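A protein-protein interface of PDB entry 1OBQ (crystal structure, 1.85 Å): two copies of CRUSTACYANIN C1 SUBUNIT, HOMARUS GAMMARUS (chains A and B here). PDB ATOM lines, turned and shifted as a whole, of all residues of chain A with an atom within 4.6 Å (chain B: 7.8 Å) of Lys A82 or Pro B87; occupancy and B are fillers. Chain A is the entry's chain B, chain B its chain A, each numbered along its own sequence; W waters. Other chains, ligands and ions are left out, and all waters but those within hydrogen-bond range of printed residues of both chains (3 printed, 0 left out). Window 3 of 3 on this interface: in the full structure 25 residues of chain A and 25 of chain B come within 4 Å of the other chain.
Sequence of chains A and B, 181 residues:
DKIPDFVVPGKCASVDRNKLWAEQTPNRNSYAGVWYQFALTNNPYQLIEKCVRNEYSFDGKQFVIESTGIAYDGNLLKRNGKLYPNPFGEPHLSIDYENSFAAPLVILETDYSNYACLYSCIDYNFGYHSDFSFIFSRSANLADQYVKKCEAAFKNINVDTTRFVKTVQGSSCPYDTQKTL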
ATOM      1  N   GLN A  62      24.912  21.851  -1.719  1.00  0.00           N
ATOM      2  CA  GLN A  62      24.697  20.465  -1.473  1.00  0.00           C
ATOM      3  C   GLN A  62      24.001  19.891  -2.693  1.00  0.00           C
ATOM      4  O   GLN A  62      23.623  20.626  -3.649  1.00  0.00           O
ATOM      5  CB  GLN A  62      23.850  20.404  -0.236  1.00  0.00           C
ATOM      6  CG  GLN A  62      22.495  21.050  -0.446  1.00  0.00           C
ATOM      7  CD  GLN A  62      21.547  20.863   0.746  1.00  0.00           C
ATOM      8  OE1 GLN A  62      20.333  20.790   0.577  1.00  0.00           O
ATOM      9  NE2 GLN A  62      22.115  20.880   1.950  1.00  0.00           N
ATOM     10  N   PHE A  63      23.828  18.590  -2.684  1.00  0.00           N
ATOM     11  CA  PHE A  63      22.973  18.046  -3.706  1.00  0.00           C
ATOM     12  C   PHE A  63      21.671  17.614  -3.060  1.00  0.00           C
ATOM     13  O   PHE A  63      21.660  17.019  -1.967  1.00  0.00           O
ATOM     14  CB  PHE A  63      23.516  16.769  -4.381  1.00  0.00           C
ATOM     15  CG  PHE A  63      24.815  16.943  -5.103  1.00  0.00           C
ATOM     16  CD1 PHE A  63      25.970  17.005  -4.400  1.00  0.00           C
ATOM     17  CD2 PHE A  63      24.855  17.118  -6.493  1.00  0.00           C
ATOM     18  CE1 PHE A  63      27.192  17.141  -5.089  1.00  0.00           C
ATOM     19  CE2 PHE A  63      26.035  17.315  -7.099  1.00  0.00           C
ATOM     20  CZ  PHE A  63      27.190  17.255  -6.387  1.00  0.00           C
ATOM     21  N   ILE A  65      18.565  14.980  -3.689  1.00  0.00           N
ATOM     22  CA  ILE A  65      18.396  13.753  -4.378  1.00  0.00           C
ATOM     23  C   ILE A  65      16.983  13.213  -4.344  1.00  0.00           C
ATOM     24  O   ILE A  65      16.363  13.170  -3.281  1.00  0.00           O
ATOM     25  CB  ILE A  65      19.319  12.686  -3.787  1.00  0.00           C
ATOM     26  CG1 ILE A  65      20.762  13.154  -3.758  1.00  0.00           C
ATOM     27  CG2 ILE A  65      19.293  11.414  -4.600  1.00  0.00           C
ATOM     28  CD1 ILE A  65      21.524  12.346  -2.749  1.00  0.00           C
ATOM     29  N   ASN A  80      13.647  10.787  -0.540  1.00  0.00           N
ATOM     30  CA  ASN A  80      14.288  12.079  -0.640  1.00  0.00           C
ATOM     31  C   ASN A  80      15.655  12.049   0.140  1.00  0.00           C
ATOM     32  O   ASN A  80      15.701  11.665   1.321  1.00  0.00           O
ATOM     33  CB  ASN A  80      13.444  13.168  -0.018  1.00  0.00           C
ATOM     34  CG  ASN A  80      12.200  13.453  -0.762  1.00  0.00           C
ATOM     35  OD1 ASN A  80      12.261  13.793  -1.947  1.00  0.00           O
ATOM     36  ND2 ASN A  80      11.048  13.373  -0.059  1.00  0.00           N
ATOM     37  N   GLY A  81      16.724  12.489  -0.501  1.00  0.00           N
ATOM     38  CA  GLY A  81      18.030  12.514   0.106  1.00  0.00           C
ATOM     39  C   GLY A  81      18.712  13.813  -0.093  1.00  0.00           C
ATOM     40  O   GLY A  81      18.321  14.674  -0.869  1.00  0.00           O
ATOM     41  N   LYS A  82      19.778  13.958   0.672  1.00  0.00           N
ATOM     42  CA  LYS A  82      20.676  15.051   0.484  1.00  0.00           C
ATOM     43  C   LYS A  82      22.105  14.561   0.548  1.00  0.00           C
ATOM     44  O   LYS A  82      22.421  13.606   1.241  1.00  0.00           O
ATOM     45  CB  LYS A  82      20.583  16.152   1.546  1.00  0.00           C
ATOM     46  CG  LYS A  82      19.318  16.946   1.593  1.00  0.00           C
ATOM     47  CD  LYS A  82      19.487  17.914   2.765  1.00  0.00           C
ATOM     48  CE  LYS A  82      18.321  18.766   3.097  1.00  0.00           C
ATOM     49  NZ  LYS A  82      17.655  19.216   1.954  1.00  0.00           N
ATOM     50  N   LEU A  83      23.001  15.321  -0.106  1.00  0.00           N
ATOM     51  CA  LEU A  83      24.407  15.006  -0.099  1.00  0.00           C
ATOM     52  C   LEU A  83      25.141  16.356   0.137  1.00  0.00           C
ATOM     53  O   LEU A  83      25.076  17.273  -0.705  1.00  0.00           O
ATOM     54  CB  LEU A  83      24.810  14.387  -1.437  1.00  0.00           C
ATOM     55  CG  LEU A  83      26.249  13.898  -1.597  1.00  0.00           C
ATOM     56  CD1 LEU A  83      26.639  12.790  -0.606  1.00  0.00           C
ATOM     57  CD2 LEU A  83      26.408  13.418  -3.025  1.00  0.00           C
ATOM     58  N   TYR A  84      25.861  16.468   1.244  1.00  0.00           N
ATOM     59  CA  TYR A  84      26.475  17.728   1.690  1.00  0.00           C
ATOM     60  C   TYR A  84      27.811  17.490   2.376  1.00  0.00           C
ATOM     61  O   TYR A  84      28.117  16.372   2.851  1.00  0.00           O
ATOM     62  CB  TYR A  84      25.448  18.487   2.554  1.00  0.00           C
ATOM     63  CG  TYR A  84      24.859  17.691   3.733  1.00  0.00           C
ATOM     64  CD1 TYR A  84      25.571  17.490   4.924  1.00  0.00           C
ATOM     65  CD2 TYR A  84      23.610  17.204   3.673  1.00  0.00           C
ATOM     66  CE1 TYR A  84      25.000  16.763   5.989  1.00  0.00           C
ATOM     67  CE2 TYR A  84      23.011  16.516   4.760  1.00  0.00           C
ATOM     68  CZ  TYR A  84      23.702  16.296   5.877  1.00  0.00           C
ATOM     69  OH  TYR A  84      23.089  15.584   6.867  1.00  0.00           O
ATOM     70  N   SER A  94      28.407  13.778   3.463  1.00  0.00           N
ATOM     71  CA  SER A  94      27.443  12.981   4.230  1.00  0.00           C
ATOM     72  C   SER A  94      26.298  12.691   3.298  1.00  0.00           C
ATOM     73  O   SER A  94      25.809  13.650   2.629  1.00  0.00           O
ATOM     74  CB  SER A  94      26.880  13.746   5.447  1.00  0.00           C
ATOM     75  OG  SER A  94      27.852  14.047   6.390  1.00  0.00           O
ATOM     76  N   ILE A  95      25.820  11.451   3.226  1.00  0.00           N
ATOM     77  CA  ILE A  95      24.602  11.152   2.452  1.00  0.00           C
ATOM     78  C   ILE A  95      23.536  10.958   3.481  1.00  0.00           C
ATOM     79  O   ILE A  95      23.707  10.122   4.414  1.00  0.00           O
ATOM     80  CB  ILE A  95      24.825   9.975   1.460  1.00  0.00           C
ATOM     81  CG1 ILE A  95      23.559   9.720   0.662  1.00  0.00           C
ATOM     82  CG2 ILE A  95      25.127   8.739   2.170  1.00  0.00           C
ATOM     83  CD1 ILE A  95      23.274  10.647  -0.453  1.00  0.00           C
ATOM     84  N   ASP A  96      22.414  11.607   3.329  1.00  0.00           N
ATOM     85  CA  ASP A  96      21.390  11.667   4.375  1.00  0.00           C
ATOM     86  C   ASP A  96      20.092  11.483   3.714  1.00  0.00           C
ATOM     87  O   ASP A  96      19.809  12.126   2.737  1.00  0.00           O
ATOM     88  CB  ASP A  96      21.591  13.043   5.010  1.00  0.00           C
ATOM     89  CG  ASP A  96      20.800  13.279   6.289  1.00  0.00           C
ATOM     90  OD1 ASP A  96      19.963  12.454   6.600  1.00  0.00           O
ATOM     91  OD2 ASP A  96      21.034  14.239   7.015  1.00  0.00           O
ATOM     92  N   TYR B  84      21.823  18.794  15.982  1.00  0.00           N
ATOM     93  CA  TYR B  84      21.189  19.848  15.194  1.00  0.00           C
ATOM     94  C   TYR B  84      19.872  19.320  14.671  1.00  0.00           C
ATOM     95  O   TYR B  84      19.684  18.098  14.523  1.00  0.00           O
ATOM     96  CB  TYR B  84      22.131  20.282  14.094  1.00  0.00           C
ATOM     97  CG  TYR B  84      22.768  19.213  13.278  1.00  0.00           C
ATOM     98  CD1 TYR B  84      22.042  18.542  12.277  1.00  0.00           C
ATOM     99  CD2 TYR B  84      24.098  18.881  13.427  1.00  0.00           C
ATOM    100  CE1 TYR B  84      22.594  17.565  11.528  1.00  0.00           C
ATOM    101  CE2 TYR B  84      24.657  17.869  12.704  1.00  0.00           C
ATOM    102  CZ  TYR B  84      23.899  17.175  11.761  1.00  0.00           C
ATOM    103  OH  TYR B  84      24.529  16.264  10.934  1.00  0.00           O
ATOM    104  N   PRO B  85      18.931  20.197  14.342  1.00  0.00           N
ATOM    105  CA  PRO B  85      17.682  19.716  13.784  1.00  0.00           C
ATOM    106  C   PRO B  85      17.890  18.907  12.552  1.00  0.00           C
ATOM    107  O   PRO B  85      18.718  19.171  11.698  1.00  0.00           O
ATOM    108  CB  PRO B  85      16.918  21.002  13.387  1.00  0.00           C
ATOM    109  CG  PRO B  85      17.625  22.113  14.097  1.00  0.00           C
ATOM    110  CD  PRO B  85      18.981  21.658  14.497  1.00  0.00           C
ATOM    111  N   ASN B  86      17.070  17.897  12.429  1.00  0.00           N
ATOM    112  CA  ASN B  86      17.123  17.065  11.216  1.00  0.00           C
ATOM    113  C   ASN B  86      17.018  17.949   9.939  1.00  0.00           C
ATOM    114  O   ASN B  86      16.154  18.868   9.875  1.00  0.00           O
ATOM    115  CB  ASN B  86      15.985  16.057  11.306  1.00  0.00           C
ATOM    116  CG  ASN B  86      15.737  15.310  10.005  1.00  0.00           C
ATOM    117  OD1 ASN B  86      15.016  15.825   9.130  1.00  0.00           O
ATOM    118  ND2 ASN B  86      16.405  14.151   9.833  1.00  0.00           N
ATOM    119  N   PRO B  87      17.910  17.754   8.959  1.00  0.00           N
ATOM    120  CA  PRO B  87      17.945  18.605   7.768  1.00  0.00           C
ATOM    121  C   PRO B  87      16.725  18.541   6.825  1.00  0.00           C
ATOM    122  O   PRO B  87      16.668  19.388   5.955  1.00  0.00           O
ATOM    123  CB  PRO B  87      19.214  18.097   7.022  1.00  0.00           C
ATOM    124  CG  PRO B  87      20.041  17.499   8.047  1.00  0.00           C
ATOM    125  CD  PRO B  87      19.058  16.810   8.959  1.00  0.00           C
ATOM    126  N   PHE B  88      15.868  17.558   6.960  1.00  0.00           N
ATOM    127  CA  PHE B  88      14.653  17.537   6.123  1.00  0.00           C
ATOM    128  C   PHE B  88      13.476  18.170   6.838  1.00  0.00           C
ATOM    129  O   PHE B  88      12.336  17.999   6.408  1.00  0.00           O
ATOM    130  CB  PHE B  88      14.294  16.134   5.633  1.00  0.00           C
ATOM    131  CG  PHE B  88      15.386  15.482   4.859  1.00  0.00           C
ATOM    132  CD1 PHE B  88      15.441  15.559   3.477  1.00  0.00           C
ATOM    133  CD2 PHE B  88      16.310  14.717   5.547  1.00  0.00           C
ATOM    134  CE1 PHE B  88      16.458  14.931   2.825  1.00  0.00           C
ATOM    135  CE2 PHE B  88      17.352  14.105   4.948  1.00  0.00           C
ATOM    136  CZ  PHE B  88      17.433  14.199   3.547  1.00  0.00           C
ATOM    137  N   GLY B  89      13.686  18.746   8.011  1.00  0.00           N
ATOM    138  CA  GLY B  89      12.580  19.360   8.763  1.00  0.00           C
ATOM    139  C   GLY B  89      11.754  18.403   9.611  1.00  0.00           C
ATOM    140  O   GLY B  89      10.699  18.819  10.121  1.00  0.00           O
ATOM    141  N   GLU B  90      12.161  17.134   9.778  1.00  0.00           N
ATOM    142  CA  GLU B  90      11.414  16.217  10.625  1.00  0.00           C
ATOM    143  C   GLU B  90      11.642  16.711  12.093  1.00  0.00           C
ATOM    144  O   GLU B  90      12.658  17.386  12.370  1.00  0.00           O
ATOM    145  CB  GLU B  90      11.870  14.731  10.488  1.00  0.00           C
ATOM    146  CG  GLU B  90      12.033  14.204   9.053  1.00  0.00           C
ATOM    147  CD  GLU B  90      12.692  12.783   9.032  1.00  0.00           C
ATOM    148  OE1 GLU B  90      12.064  11.860   9.649  1.00  0.00           O
ATOM    149  OE2 GLU B  90      13.857  12.553   8.448  1.00  0.00           O
ATOM    150  N   HIS B  92      12.769  16.036  14.823  1.00  0.00           N
ATOM    151  CA  HIS B  92      13.811  15.380  15.665  1.00  0.00           C
ATOM    152  C   HIS B  92      15.172  15.916  15.346  1.00  0.00           C
ATOM    153  O   HIS B  92      15.364  16.653  14.412  1.00  0.00           O
ATOM    154  CB  HIS B  92      13.784  13.848  15.650  1.00  0.00           C
ATOM    155  CG  HIS B  92      13.968  13.222  14.295  1.00  0.00           C
ATOM    156  ND1 HIS B  92      15.197  13.010  13.704  1.00  0.00           N
ATOM    157  CD2 HIS B  92      13.047  12.739  13.424  1.00  0.00           C
ATOM    158  CE1 HIS B  92      15.025  12.400  12.527  1.00  0.00           C
ATOM    159  NE2 HIS B  92      13.720  12.224  12.342  1.00  0.00           N
ATOM    160  N   LEU B  93      16.145  15.518  16.140  1.00  0.00           N
ATOM    161  CA  LEU B  93      17.492  16.055  16.050  1.00  0.00           C
ATOM    162  C   LEU B  93      18.362  14.991  15.419  1.00  0.00           C
ATOM    163  O   LEU B  93      18.054  13.834  15.435  1.00  0.00           O
ATOM    164  CB  LEU B  93      18.015  16.379  17.468  1.00  0.00           C
ATOM    165  CG  LEU B  93      17.336  17.497  18.258  1.00  0.00           C
ATOM    166  CD1 LEU B  93      17.685  17.331  19.798  1.00  0.00           C
ATOM    167  CD2 LEU B  93      17.712  18.809  17.647  1.00  0.00           C
ATOM    168  N   SER B  94      19.468  15.400  14.835  1.00  0.00           N
ATOM    169  CA  SER B  94      20.443  14.458  14.413  1.00  0.00           C
ATOM    170  C   SER B  94      21.589  14.542  15.403  1.00  0.00           C
ATOM    171  O   SER B  94      22.054  15.639  15.688  1.00  0.00           O
ATOM    172  CB  SER B  94      20.970  14.876  13.018  1.00  0.00           C
ATOM    173  OG  SER B  94      19.975  14.746  12.024  1.00  0.00           O
ATOM    174  N   ALA B 102      25.739  10.059  11.489  1.00  0.00           N
ATOM    175  CA  ALA B 102      24.676  10.732  12.233  1.00  0.00           C
ATOM    176  C   ALA B 102      23.404   9.912  12.282  1.00  0.00           C
ATOM    177  O   ALA B 102      23.065   9.228  11.294  1.00  0.00           O
ATOM    178  CB  ALA B 102      24.386  12.089  11.647  1.00  0.00           C
HETATM  179  O   HOH W   1      23.963  14.698   9.189  1.00  0.00           O
HETATM  180  O   HOH W   2      17.577  12.092   7.952  1.00  0.00           O
HETATM  181  O   HOH W   3      21.272  14.164   9.617  1.00  0.00           O
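Ile A65 touches none of the printed residues of chain B. Of the printed residues of chain B, Asn A80 touches Phe B88 (3.7 Å). Of chain B, only Phe B88 (3.9 Å) comes within 4 Å of Gly A81. Lys A82 touches just these residues of chain B: Pro B87 and Phe B88. Of the printed residues of chain B, Tyr A84 touches Pro B87 (3.8 Å). Tyr B84 touches none of the printed residues of chain A. Of chain A, only Lys A82, Tyr A84 and Asp A96 come within 4 Å of Pro B87.
Of the 11 printed residues of chain A, 5 touch a printed residue of chain B. Printed residues of chain A that touch a printed residue of chain B: Asn A80, Gly A81, Lys A82, Tyr A84 and Asp A96. Hydrophobic or aromatic side chains of chain B within 4 Å of the printed part of chain A: Pro B87 and Phe B88. Along chain B the printed residues that touch a printed residue of chain A span positions 87 to 88. Among the printed residues, 7 pairs touch across the chains. Among the printed residues, no Asp or Glu carboxylate lies within 4 Å of a Lys or Arg side-chain nitrogen of the other chain.
Positions printed for both chains: 84 and 94.
Water W1 bridges OH of Tyr B84 (2.4 Å) and OH of Tyr A84 (2.6 Å). Water W3 lies within hydrogen-bond range of the side-chain carboxylate of Asp A96 and the side-chain hydroxyl of Ser B94. Water W2 lies within hydrogen-bond range of OD1 of Asp A96 (2.8 Å) and ND2 of Asn B86 (3.0 Å).
Among the printed residues, pairs that only touch across the chains: Asn A80 with Phe B88 (3.7 Å), Gly A81 with Phe B88 (3.9 Å), Lys A82 with Pro B87 (3.4 Å), Lys A82 with Phe B88 (3.7 Å), Tyr A84 with Pro B87 (3.8 Å), Asp A96 with Pro B87 (3.6 Å) and Asp A96 with Phe B88 (3.3 Å).
The backbone NH (N) of Ile A65 is in hydrogen-bond range of the backbone carbonyl oxygen (O) of Gly A81 (2.8 Å). The side-chain amide oxygen of Gln A62 is in hydrogen-bond range of the side-chain amino group of Lys A82 (3.4 Å). The backbone carbonyl oxygen of Asp A96 is in hydrogen-bond range of the backbone NH of Lys A82, 2.8 Å away. N of Phe B88 sits at hydrogen-bond distance from OD1 of Asn B86 (2.9 Å). The backbone carbonyl oxygen (O) of Tyr A84 sits at hydrogen-bond distance from the backbone NH (N) of Ser A94 (2.7 Å). OH of Tyr A84 is in hydrogen-bond range of OD2 of Asp A96 (2.5 Å).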
